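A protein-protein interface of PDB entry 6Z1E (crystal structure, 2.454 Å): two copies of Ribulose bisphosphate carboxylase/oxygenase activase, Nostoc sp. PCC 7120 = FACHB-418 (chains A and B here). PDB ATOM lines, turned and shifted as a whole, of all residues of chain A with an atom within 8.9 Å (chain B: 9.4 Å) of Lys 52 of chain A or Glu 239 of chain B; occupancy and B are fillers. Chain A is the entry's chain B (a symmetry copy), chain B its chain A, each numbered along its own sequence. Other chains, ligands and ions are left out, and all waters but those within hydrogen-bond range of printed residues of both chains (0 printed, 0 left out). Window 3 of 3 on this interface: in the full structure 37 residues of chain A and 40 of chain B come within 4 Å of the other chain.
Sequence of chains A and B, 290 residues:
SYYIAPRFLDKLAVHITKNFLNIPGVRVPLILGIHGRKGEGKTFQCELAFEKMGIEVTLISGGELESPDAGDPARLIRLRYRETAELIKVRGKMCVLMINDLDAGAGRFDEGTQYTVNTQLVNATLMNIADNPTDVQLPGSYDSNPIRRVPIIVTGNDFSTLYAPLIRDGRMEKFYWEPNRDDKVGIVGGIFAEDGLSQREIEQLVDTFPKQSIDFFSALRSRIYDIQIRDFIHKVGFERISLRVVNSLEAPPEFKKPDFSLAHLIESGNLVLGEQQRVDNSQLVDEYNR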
ATOM      1  N   SER A   1      26.527  27.708 -11.459  1.00  0.00           N
ATOM      2  CA  SER A   1      25.380  27.000 -12.016  1.00  0.00           C
ATOM      3  C   SER A   1      25.780  26.257 -13.288  1.00  0.00           C
ATOM      4  O   SER A   1      26.406  26.828 -14.179  1.00  0.00           O
ATOM      5  CB  SER A   1      24.248  27.980 -12.318  1.00  0.00           C
ATOM      6  OG  SER A   1      23.076  27.298 -12.731  1.00  0.00           O
ATOM      7  N   TYR A   2      25.412  24.982 -13.362  1.00  0.00           N
ATOM      8  CA  TYR A   2      25.815  24.130 -14.476  1.00  0.00           C
ATOM      9  C   TYR A   2      24.903  24.291 -15.682  1.00  0.00           C
ATOM     10  O   TYR A   2      23.688  24.432 -15.548  1.00  0.00           O
ATOM     11  CB  TYR A   2      25.866  22.667 -14.031  1.00  0.00           C
ATOM     12  CG  TYR A   2      26.953  22.390 -13.018  1.00  0.00           C
ATOM     13  CD1 TYR A   2      28.228  22.915 -13.181  1.00  0.00           C
ATOM     14  CD2 TYR A   2      26.703  21.612 -11.895  1.00  0.00           C
ATOM     15  CE1 TYR A   2      29.226  22.674 -12.262  1.00  0.00           C
ATOM     16  CE2 TYR A   2      27.696  21.365 -10.964  1.00  0.00           C
ATOM     17  CZ  TYR A   2      28.955  21.899 -11.152  1.00  0.00           C
ATOM     18  OH  TYR A   2      29.953  21.659 -10.234  1.00  0.00           O
ATOM     19  N   ILE A   4      23.100  23.278 -19.212  1.00  0.00           N
ATOM     20  CA  ILE A   4      22.538  22.218 -20.041  1.00  0.00           C
ATOM     21  C   ILE A   4      22.413  22.751 -21.466  1.00  0.00           C
ATOM     22  O   ILE A   4      21.890  23.843 -21.680  1.00  0.00           O
ATOM     23  CB  ILE A   4      21.160  21.732 -19.502  1.00  0.00           C
ATOM     24  CG1 ILE A   4      20.528  20.704 -20.442  1.00  0.00           C
ATOM     25  CG2 ILE A   4      20.198  22.898 -19.303  1.00  0.00           C
ATOM     26  CD1 ILE A   4      21.301  19.417 -20.547  1.00  0.00           C
ATOM     27  N   LEU A   9      18.691  19.292 -24.039  1.00  0.00           N
ATOM     28  CA  LEU A   9      17.494  19.373 -23.209  1.00  0.00           C
ATOM     29  C   LEU A   9      16.231  19.118 -24.034  1.00  0.00           C
ATOM     30  O   LEU A   9      15.337  18.399 -23.593  1.00  0.00           O
ATOM     31  CB  LEU A   9      17.415  20.740 -22.518  1.00  0.00           C
ATOM     32  CG  LEU A   9      16.186  21.000 -21.638  1.00  0.00           C
ATOM     33  CD1 LEU A   9      16.048  19.945 -20.543  1.00  0.00           C
ATOM     34  CD2 LEU A   9      16.253  22.395 -21.031  1.00  0.00           C
ATOM     35  N   ALA A  13      13.814  15.877 -23.508  1.00  0.00           N
ATOM     36  CA  ALA A  13      12.487  16.237 -23.020  1.00  0.00           C
ATOM     37  C   ALA A  13      11.399  15.808 -24.003  1.00  0.00           C
ATOM     38  O   ALA A  13      10.343  15.325 -23.590  1.00  0.00           O
ATOM     39  CB  ALA A  13      12.411  17.731 -22.761  1.00  0.00           C
ATOM     40  N   GLN A  45      24.387  15.716 -18.339  1.00  0.00           N
ATOM     41  CA  GLN A  45      23.320  16.554 -18.875  1.00  0.00           C
ATOM     42  C   GLN A  45      21.960  15.878 -18.785  1.00  0.00           C
ATOM     43  O   GLN A  45      20.932  16.551 -18.714  1.00  0.00           O
ATOM     44  CB  GLN A  45      23.602  16.918 -20.326  1.00  0.00           C
ATOM     45  CG  GLN A  45      24.673  17.965 -20.486  1.00  0.00           C
ATOM     46  CD  GLN A  45      24.885  18.329 -21.931  1.00  0.00           C
ATOM     47  OE1 GLN A  45      24.630  19.459 -22.345  1.00  0.00           O
ATOM     48  NE2 GLN A  45      25.343  17.365 -22.716  1.00  0.00           N
ATOM     49  N   CYS A  46      21.952  14.550 -18.816  1.00  0.00           N
ATOM     50  CA  CYS A  46      20.722  13.813 -18.592  1.00  0.00           C
ATOM     51  C   CYS A  46      20.222  14.149 -17.193  1.00  0.00           C
ATOM     52  O   CYS A  46      19.043  14.441 -16.995  1.00  0.00           O
ATOM     53  CB  CYS A  46      20.947  12.305 -18.736  1.00  0.00           C
ATOM     54  SG  CYS A  46      20.837  11.681 -20.429  1.00  0.00           S
ATOM     55  N   GLU A  47      21.139  14.136 -16.229  1.00  0.00           N
ATOM     56  CA  GLU A  47      20.799  14.413 -14.840  1.00  0.00           C
ATOM     57  C   GLU A  47      20.348  15.857 -14.640  1.00  0.00           C
ATOM     58  O   GLU A  47      19.459  16.124 -13.834  1.00  0.00           O
ATOM     59  CB  GLU A  47      21.981  14.089 -13.921  1.00  0.00           C
ATOM     60  CG  GLU A  47      22.238  12.592 -13.795  1.00  0.00           C
ATOM     61  CD  GLU A  47      23.395  12.258 -12.874  1.00  0.00           C
ATOM     62  OE1 GLU A  47      24.192  13.163 -12.552  1.00  0.00           O
ATOM     63  OE2 GLU A  47      23.505  11.079 -12.474  1.00  0.00           O
ATOM     64  N   LEU A  48      20.957  16.785 -15.370  1.00  0.00           N
ATOM     65  CA  LEU A  48      20.552  18.182 -15.292  1.00  0.00           C
ATOM     66  C   LEU A  48      19.113  18.347 -15.773  1.00  0.00           C
ATOM     67  O   LEU A  48      18.337  19.089 -15.178  1.00  0.00           O
ATOM     68  CB  LEU A  48      21.501  19.071 -16.106  1.00  0.00           C
ATOM     69  CG  LEU A  48      22.898  19.265 -15.503  1.00  0.00           C
ATOM     70  CD1 LEU A  48      23.774  20.071 -16.452  1.00  0.00           C
ATOM     71  CD2 LEU A  48      22.850  19.931 -14.129  1.00  0.00           C
ATOM     72  N   ALA A  49      18.759  17.639 -16.839  1.00  0.00           N
ATOM     73  CA  ALA A  49      17.427  17.741 -17.424  1.00  0.00           C
ATOM     74  C   ALA A  49      16.365  17.123 -16.515  1.00  0.00           C
ATOM     75  O   ALA A  49      15.265  17.661 -16.381  1.00  0.00           O
ATOM     76  CB  ALA A  49      17.400  17.078 -18.789  1.00  0.00           C
ATOM     77  N   PHE A  50      16.693  15.988 -15.903  1.00  0.00           N
ATOM     78  CA  PHE A  50      15.780  15.331 -14.973  1.00  0.00           C
ATOM     79  C   PHE A  50      15.508  16.225 -13.770  1.00  0.00           C
ATOM     80  O   PHE A  50      14.383  16.284 -13.273  1.00  0.00           O
ATOM     81  CB  PHE A  50      16.364  13.995 -14.502  1.00  0.00           C
ATOM     82  CG  PHE A  50      16.567  12.992 -15.605  1.00  0.00           C
ATOM     83  CD1 PHE A  50      15.775  13.010 -16.744  1.00  0.00           C
ATOM     84  CD2 PHE A  50      17.555  12.027 -15.502  1.00  0.00           C
ATOM     85  CE1 PHE A  50      15.965  12.086 -17.753  1.00  0.00           C
ATOM     86  CE2 PHE A  50      17.749  11.102 -16.510  1.00  0.00           C
ATOM     87  CZ  PHE A  50      16.953  11.131 -17.637  1.00  0.00           C
ATOM     88  N   GLU A  51      16.543  16.917 -13.304  1.00  0.00           N
ATOM     89  CA  GLU A  51      16.399  17.846 -12.193  1.00  0.00           C
ATOM     90  C   GLU A  51      15.534  19.021 -12.627  1.00  0.00           C
ATOM     91  O   GLU A  51      14.660  19.473 -11.888  1.00  0.00           O
ATOM     92  CB  GLU A  51      17.768  18.345 -11.733  1.00  0.00           C
ATOM     93  N   LYS A  52      15.791  19.506 -13.837  1.00  0.00           N
ATOM     94  CA  LYS A  52      15.059  20.634 -14.400  1.00  0.00           C
ATOM     95  C   LYS A  52      13.574  20.303 -14.500  1.00  0.00           C
ATOM     96  O   LYS A  52      12.723  21.131 -14.182  1.00  0.00           O
ATOM     97  CB  LYS A  52      15.616  20.972 -15.788  1.00  0.00           C
ATOM     98  CG  LYS A  52      14.966  22.170 -16.482  1.00  0.00           C
ATOM     99  CD  LYS A  52      15.725  23.463 -16.217  1.00  0.00           C
ATOM    100  CE  LYS A  52      15.210  24.597 -17.093  1.00  0.00           C
ATOM    101  NZ  LYS A  52      15.955  25.867 -16.870  1.00  0.00           N
ATOM    102  N   MET A  53      13.274  19.083 -14.932  1.00  0.00           N
ATOM    103  CA  MET A  53      11.895  18.662 -15.165  1.00  0.00           C
ATOM    104  C   MET A  53      11.300  17.934 -13.965  1.00  0.00           C
ATOM    105  O   MET A  53      10.161  17.468 -14.018  1.00  0.00           O
ATOM    106  CB  MET A  53      11.825  17.769 -16.404  1.00  0.00           C
ATOM    107  CG  MET A  53      12.161  18.497 -17.692  1.00  0.00           C
ATOM    108  SD  MET A  53      12.061  17.428 -19.137  1.00  0.00           S
ATOM    109  CE  MET A  53      13.614  16.557 -19.012  1.00  0.00           C
ATOM    110  N   GLY A  54      12.068  17.836 -12.884  1.00  0.00           N
ATOM    111  CA  GLY A  54      11.599  17.186 -11.674  1.00  0.00           C
ATOM    112  C   GLY A  54      11.275  15.727 -11.917  1.00  0.00           C
ATOM    113  O   GLY A  54      10.371  15.171 -11.297  1.00  0.00           O
ATOM    114  N   ILE A  55      12.018  15.108 -12.828  1.00  0.00           N
ATOM    115  CA  ILE A  55      11.815  13.707 -13.161  1.00  0.00           C
ATOM    116  C   ILE A  55      12.624  12.821 -12.227  1.00  0.00           C
ATOM    117  O   ILE A  55      13.829  13.009 -12.060  1.00  0.00           O
ATOM    118  CB  ILE A  55      12.216  13.417 -14.619  1.00  0.00           C
ATOM    119  CG1 ILE A  55      11.280  14.166 -15.569  1.00  0.00           C
ATOM    120  CG2 ILE A  55      12.164  11.913 -14.915  1.00  0.00           C
ATOM    121  CD1 ILE A  55      11.732  14.165 -17.004  1.00  0.00           C
ATOM    122  N   GLU A  56      11.943  11.858 -11.617  1.00  0.00           N
ATOM    123  CA  GLU A  56      12.607  10.852 -10.805  1.00  0.00           C
ATOM    124  C   GLU A  56      13.136   9.785 -11.755  1.00  0.00           C
ATOM    125  O   GLU A  56      12.409   9.319 -12.632  1.00  0.00           O
ATOM    126  CB  GLU A  56      11.625  10.239  -9.808  1.00  0.00           C
ATOM    127  CG  GLU A  56      12.284   9.577  -8.606  1.00  0.00           C
ATOM    128  CD  GLU A  56      13.026  10.567  -7.723  1.00  0.00           C
ATOM    129  OE1 GLU A  56      12.754  11.783  -7.834  1.00  0.00           O
ATOM    130  OE2 GLU A  56      13.881  10.125  -6.924  1.00  0.00           O
ATOM    131  N   LYS A  93       3.788  11.151 -11.607  1.00  0.00           N
ATOM    132  CA  LYS A  93       4.747  12.041 -12.255  1.00  0.00           C
ATOM    133  C   LYS A  93       5.466  11.277 -13.353  1.00  0.00           C
ATOM    134  O   LYS A  93       5.393  10.051 -13.411  1.00  0.00           O
ATOM    135  CB  LYS A  93       5.781  12.547 -11.249  1.00  0.00           C
ATOM    136  CG  LYS A  93       5.217  13.324 -10.076  1.00  0.00           C
ATOM    137  CD  LYS A  93       6.234  13.386  -8.948  1.00  0.00           C
ATOM    138  CE  LYS A  93       5.734  14.211  -7.777  1.00  0.00           C
ATOM    139  NZ  LYS A  93       5.811  15.671  -8.048  1.00  0.00           N
ATOM    140  N   MET A  94       6.163  12.002 -14.221  1.00  0.00           N
ATOM    141  CA  MET A  94       6.995  11.361 -15.229  1.00  0.00           C
ATOM    142  C   MET A  94       8.178  10.670 -14.555  1.00  0.00           C
ATOM    143  O   MET A  94       8.875  11.271 -13.740  1.00  0.00           O
ATOM    144  CB  MET A  94       7.498  12.387 -16.246  1.00  0.00           C
ATOM    145  CG  MET A  94       6.397  13.050 -17.063  1.00  0.00           C
ATOM    146  SD  MET A  94       7.021  13.964 -18.492  1.00  0.00           S
ATOM    147  CE  MET A  94       8.220  15.052 -17.734  1.00  0.00           C
ATOM    148  N   ILE B 233       6.390  21.997 -25.028  1.00  0.00           N
ATOM    149  CA  ILE B 233       7.145  21.891 -23.784  1.00  0.00           C
ATOM    150  C   ILE B 233       7.660  23.259 -23.364  1.00  0.00           C
ATOM    151  O   ILE B 233       7.695  23.586 -22.177  1.00  0.00           O
ATOM    152  CB  ILE B 233       8.337  20.927 -23.941  1.00  0.00           C
ATOM    153  CG1 ILE B 233       7.832  19.501 -24.159  1.00  0.00           C
ATOM    154  CG2 ILE B 233       9.247  20.964 -22.713  1.00  0.00           C
ATOM    155  CD1 ILE B 233       8.846  18.596 -24.811  1.00  0.00           C
ATOM    156  N   HIS B 234       8.064  24.053 -24.350  1.00  0.00           N
ATOM    157  CA  HIS B 234       8.586  25.387 -24.091  1.00  0.00           C
ATOM    158  C   HIS B 234       7.505  26.310 -23.527  1.00  0.00           C
ATOM    159  O   HIS B 234       7.754  27.062 -22.583  1.00  0.00           O
ATOM    160  CB  HIS B 234       9.181  25.977 -25.371  1.00  0.00           C
ATOM    161  CG  HIS B 234      10.492  25.370 -25.764  1.00  0.00           C
ATOM    162  ND1 HIS B 234      11.594  25.381 -24.936  1.00  0.00           N
ATOM    163  CD2 HIS B 234      10.881  24.742 -26.899  1.00  0.00           C
ATOM    164  CE1 HIS B 234      12.603  24.780 -25.541  1.00  0.00           C
ATOM    165  NE2 HIS B 234      12.196  24.383 -26.734  1.00  0.00           N
ATOM    166  N   LYS B 235       6.307  26.245 -24.102  1.00  0.00           N
ATOM    167  CA  LYS B 235       5.191  27.078 -23.657  1.00  0.00           C
ATOM    168  C   LYS B 235       4.814  26.759 -22.213  1.00  0.00           C
ATOM    169  O   LYS B 235       4.665  27.661 -21.387  1.00  0.00           O
ATOM    170  CB  LYS B 235       3.974  26.872 -24.564  1.00  0.00           C
ATOM    171  CG  LYS B 235       2.800  27.799 -24.255  1.00  0.00           C
ATOM    172  CD  LYS B 235       1.619  27.541 -25.183  1.00  0.00           C
ATOM    173  CE  LYS B 235       0.458  28.482 -24.887  1.00  0.00           C
ATOM    174  NZ  LYS B 235      -0.703  28.259 -25.797  1.00  0.00           N
ATOM    175  N   VAL B 236       4.659  25.473 -21.920  1.00  0.00           N
ATOM    176  CA  VAL B 236       4.315  25.025 -20.577  1.00  0.00           C
ATOM    177  C   VAL B 236       5.484  25.251 -19.621  1.00  0.00           C
ATOM    178  O   VAL B 236       5.284  25.526 -18.438  1.00  0.00           O
ATOM    179  CB  VAL B 236       3.922  23.530 -20.577  1.00  0.00           C
ATOM    180  CG1 VAL B 236       3.663  23.025 -19.159  1.00  0.00           C
ATOM    181  CG2 VAL B 236       2.692  23.310 -21.449  1.00  0.00           C
ATOM    182  N   GLY B 237       6.702  25.135 -20.143  1.00  0.00           N
ATOM    183  CA  GLY B 237       7.900  25.302 -19.340  1.00  0.00           C
ATOM    184  C   GLY B 237       8.369  23.980 -18.761  1.00  0.00           C
ATOM    185  O   GLY B 237       7.556  23.159 -18.332  1.00  0.00           O
ATOM    186  N   PHE B 238       9.683  23.778 -18.745  1.00  0.00           N
ATOM    187  CA  PHE B 238      10.261  22.512 -18.305  1.00  0.00           C
ATOM    188  C   PHE B 238       9.916  22.181 -16.855  1.00  0.00           C
ATOM    189  O   PHE B 238       9.878  21.013 -16.472  1.00  0.00           O
ATOM    190  CB  PHE B 238      11.783  22.536 -18.477  1.00  0.00           C
ATOM    191  CG  PHE B 238      12.232  22.561 -19.910  1.00  0.00           C
ATOM    192  CD1 PHE B 238      12.243  21.402 -20.666  1.00  0.00           C
ATOM    193  CD2 PHE B 238      12.647  23.744 -20.499  1.00  0.00           C
ATOM    194  CE1 PHE B 238      12.656  21.421 -21.985  1.00  0.00           C
ATOM    195  CE2 PHE B 238      13.060  23.770 -21.818  1.00  0.00           C
ATOM    196  CZ  PHE B 238      13.064  22.606 -22.564  1.00  0.00           C
ATOM    197  N   GLU B 239       9.658  23.209 -16.054  1.00  0.00           N
ATOM    198  CA  GLU B 239       9.395  23.022 -14.632  1.00  0.00           C
ATOM    199  C   GLU B 239       8.036  22.374 -14.358  1.00  0.00           C
ATOM    200  O   GLU B 239       7.845  21.755 -13.310  1.00  0.00           O
ATOM    201  CB  GLU B 239       9.477  24.366 -13.900  1.00  0.00           C
ATOM    202  N   ARG B 240       7.100  22.518 -15.293  1.00  0.00           N
ATOM    203  CA  ARG B 240       5.713  22.108 -15.065  1.00  0.00           C
ATOM    204  C   ARG B 240       5.193  21.115 -16.099  1.00  0.00           C
ATOM    205  O   ARG B 240       4.006  20.792 -16.103  1.00  0.00           O
ATOM    206  CB  ARG B 240       4.806  23.344 -15.053  1.00  0.00           C
ATOM    207  N   ILE B 241       6.069  20.623 -16.968  1.00  0.00           N
ATOM    208  CA  ILE B 241       5.635  19.747 -18.050  1.00  0.00           C
ATOM    209  C   ILE B 241       5.129  18.404 -17.526  1.00  0.00           C
ATOM    210  O   ILE B 241       4.197  17.824 -18.082  1.00  0.00           O
ATOM    211  CB  ILE B 241       6.765  19.504 -19.086  1.00  0.00           C
ATOM    212  CG1 ILE B 241       6.268  18.637 -20.249  1.00  0.00           C
ATOM    213  CG2 ILE B 241       7.980  18.852 -18.429  1.00  0.00           C
ATOM    214  CD1 ILE B 241       5.099  19.232 -21.013  1.00  0.00           C
ATOM    215  N   SER B 242       5.748  17.915 -16.457  1.00  0.00           N
ATOM    216  CA  SER B 242       5.387  16.623 -15.885  1.00  0.00           C
ATOM    217  C   SER B 242       3.947  16.628 -15.365  1.00  0.00           C
ATOM    218  O   SER B 242       3.186  15.696 -15.623  1.00  0.00           O
ATOM    219  CB  SER B 242       6.358  16.254 -14.759  1.00  0.00           C
ATOM    220  OG  SER B 242       6.187  14.909 -14.352  1.00  0.00           O
ATOM    221  N   LEU B 243       3.580  17.679 -14.634  1.00  0.00           N
ATOM    222  CA  LEU B 243       2.227  17.817 -14.102  1.00  0.00           C
ATOM    223  C   LEU B 243       1.208  17.926 -15.229  1.00  0.00           C
ATOM    224  O   LEU B 243       0.129  17.336 -15.162  1.00  0.00           O
ATOM    225  CB  LEU B 243       2.130  19.055 -13.200  1.00  0.00           C
ATOM    226  CG  LEU B 243       0.732  19.489 -12.729  1.00  0.00           C
ATOM    227  CD1 LEU B 243       0.094  18.428 -11.849  1.00  0.00           C
ATOM    228  CD2 LEU B 243       0.785  20.825 -11.996  1.00  0.00           C
ATOM    229  N   ARG B 244       1.558  18.680 -16.264  1.00  0.00           N
ATOM    230  CA  ARG B 244       0.629  18.981 -17.347  1.00  0.00           C
ATOM    231  C   ARG B 244       0.206  17.730 -18.109  1.00  0.00           C
ATOM    232  O   ARG B 244      -0.947  17.612 -18.525  1.00  0.00           O
ATOM    233  CB  ARG B 244       1.265  19.979 -18.316  1.00  0.00           C
ATOM    234  CG  ARG B 244       0.391  20.348 -19.508  1.00  0.00           C
ATOM    235  CD  ARG B 244      -0.895  21.035 -19.080  1.00  0.00           C
ATOM    236  NE  ARG B 244      -1.672  21.475 -20.236  1.00  0.00           N
ATOM    237  CZ  ARG B 244      -2.553  20.720 -20.886  1.00  0.00           C
ATOM    238  NH1 ARG B 244      -2.790  19.473 -20.500  1.00  0.00           N
ATOM    239  NH2 ARG B 244      -3.203  21.217 -21.929  1.00  0.00           N
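Leu 9 of chain A touches Phe 238 of chain B (CD2 to CZ, 3.5 Å).
O of Ala 13 of chain A touches CD1 of Ile 233 of chain B, 3.8 Å away.
Ala 13 of chain A touches Phe 238 of chain B (CB to CE1, 3.8 Å).
Lys 52 of chain A touches Phe 238 of chain B.
Lys 52 of chain A touches Glu 239 of chain B (O to CA, 3.9 Å).
O of Phe 238 of chain B touches CA of Met 53 of chain A (3.4 Å).
Lys 93 of chain A touches Ser 242 of chain B.
Ile 241 of chain B touches Met 94 of chain A.
No position is printed for both chains.
Of the 9 pairs that touch across the chains among the printed residues, none has its exchanged pair printed and touching as well.
Of the 19 printed residues of chain A, 6 touch a printed residue of chain B.
Hydrophobic or aromatic side chains of chain B within 4 Å of the printed part of chain A: Ile 233, Phe 238 and Ile 241.
Among the printed residues, no Asp or Glu carboxylate lies within 4 Å of a Lys or Arg side-chain nitrogen of the other chain.
Printed residues of chain B within 4 Å of Leu 9 of chain A: Phe 238.
Leu 48 of chain A touches none of the printed residues of chain B.
Glu 51 of chain A touches none of the printed residues of chain B.
Printed residues of chain B within 4 Å of Met 53 of chain A: Phe 238 (3.4 Å).
Of the printed residues of chain A, Ile 233 of chain B touches Ala 13.
Printed residues of chain A within 4 Å of Phe 238 of chain B: Leu 9, Ala 13, Lys 52 and Met 53.
Of the printed residues of chain A, Glu 239 of chain B touches Lys 52.
Printed residues of chain A within 4 Å of Ser 242 of chain B: Lys 93 and Met 94.
The nearest residue of chain B that does not touch Lys 52 of chain A is Arg 240 of chain B (5.9 Å).
The nearest residue of chain A that does not touch Glu 239 of chain B is Met 53 of chain A (4.9 Å).
The nearest printed residue of chain B that does not touch Lys 93 of chain A is Leu 243 of chain B (6.2 Å).
The side-chain hydroxyl (OG) of Ser 242 of chain B lies within hydrogen-bond range of the backbone NH (N) of Met 94 of chain A (2.9 Å).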
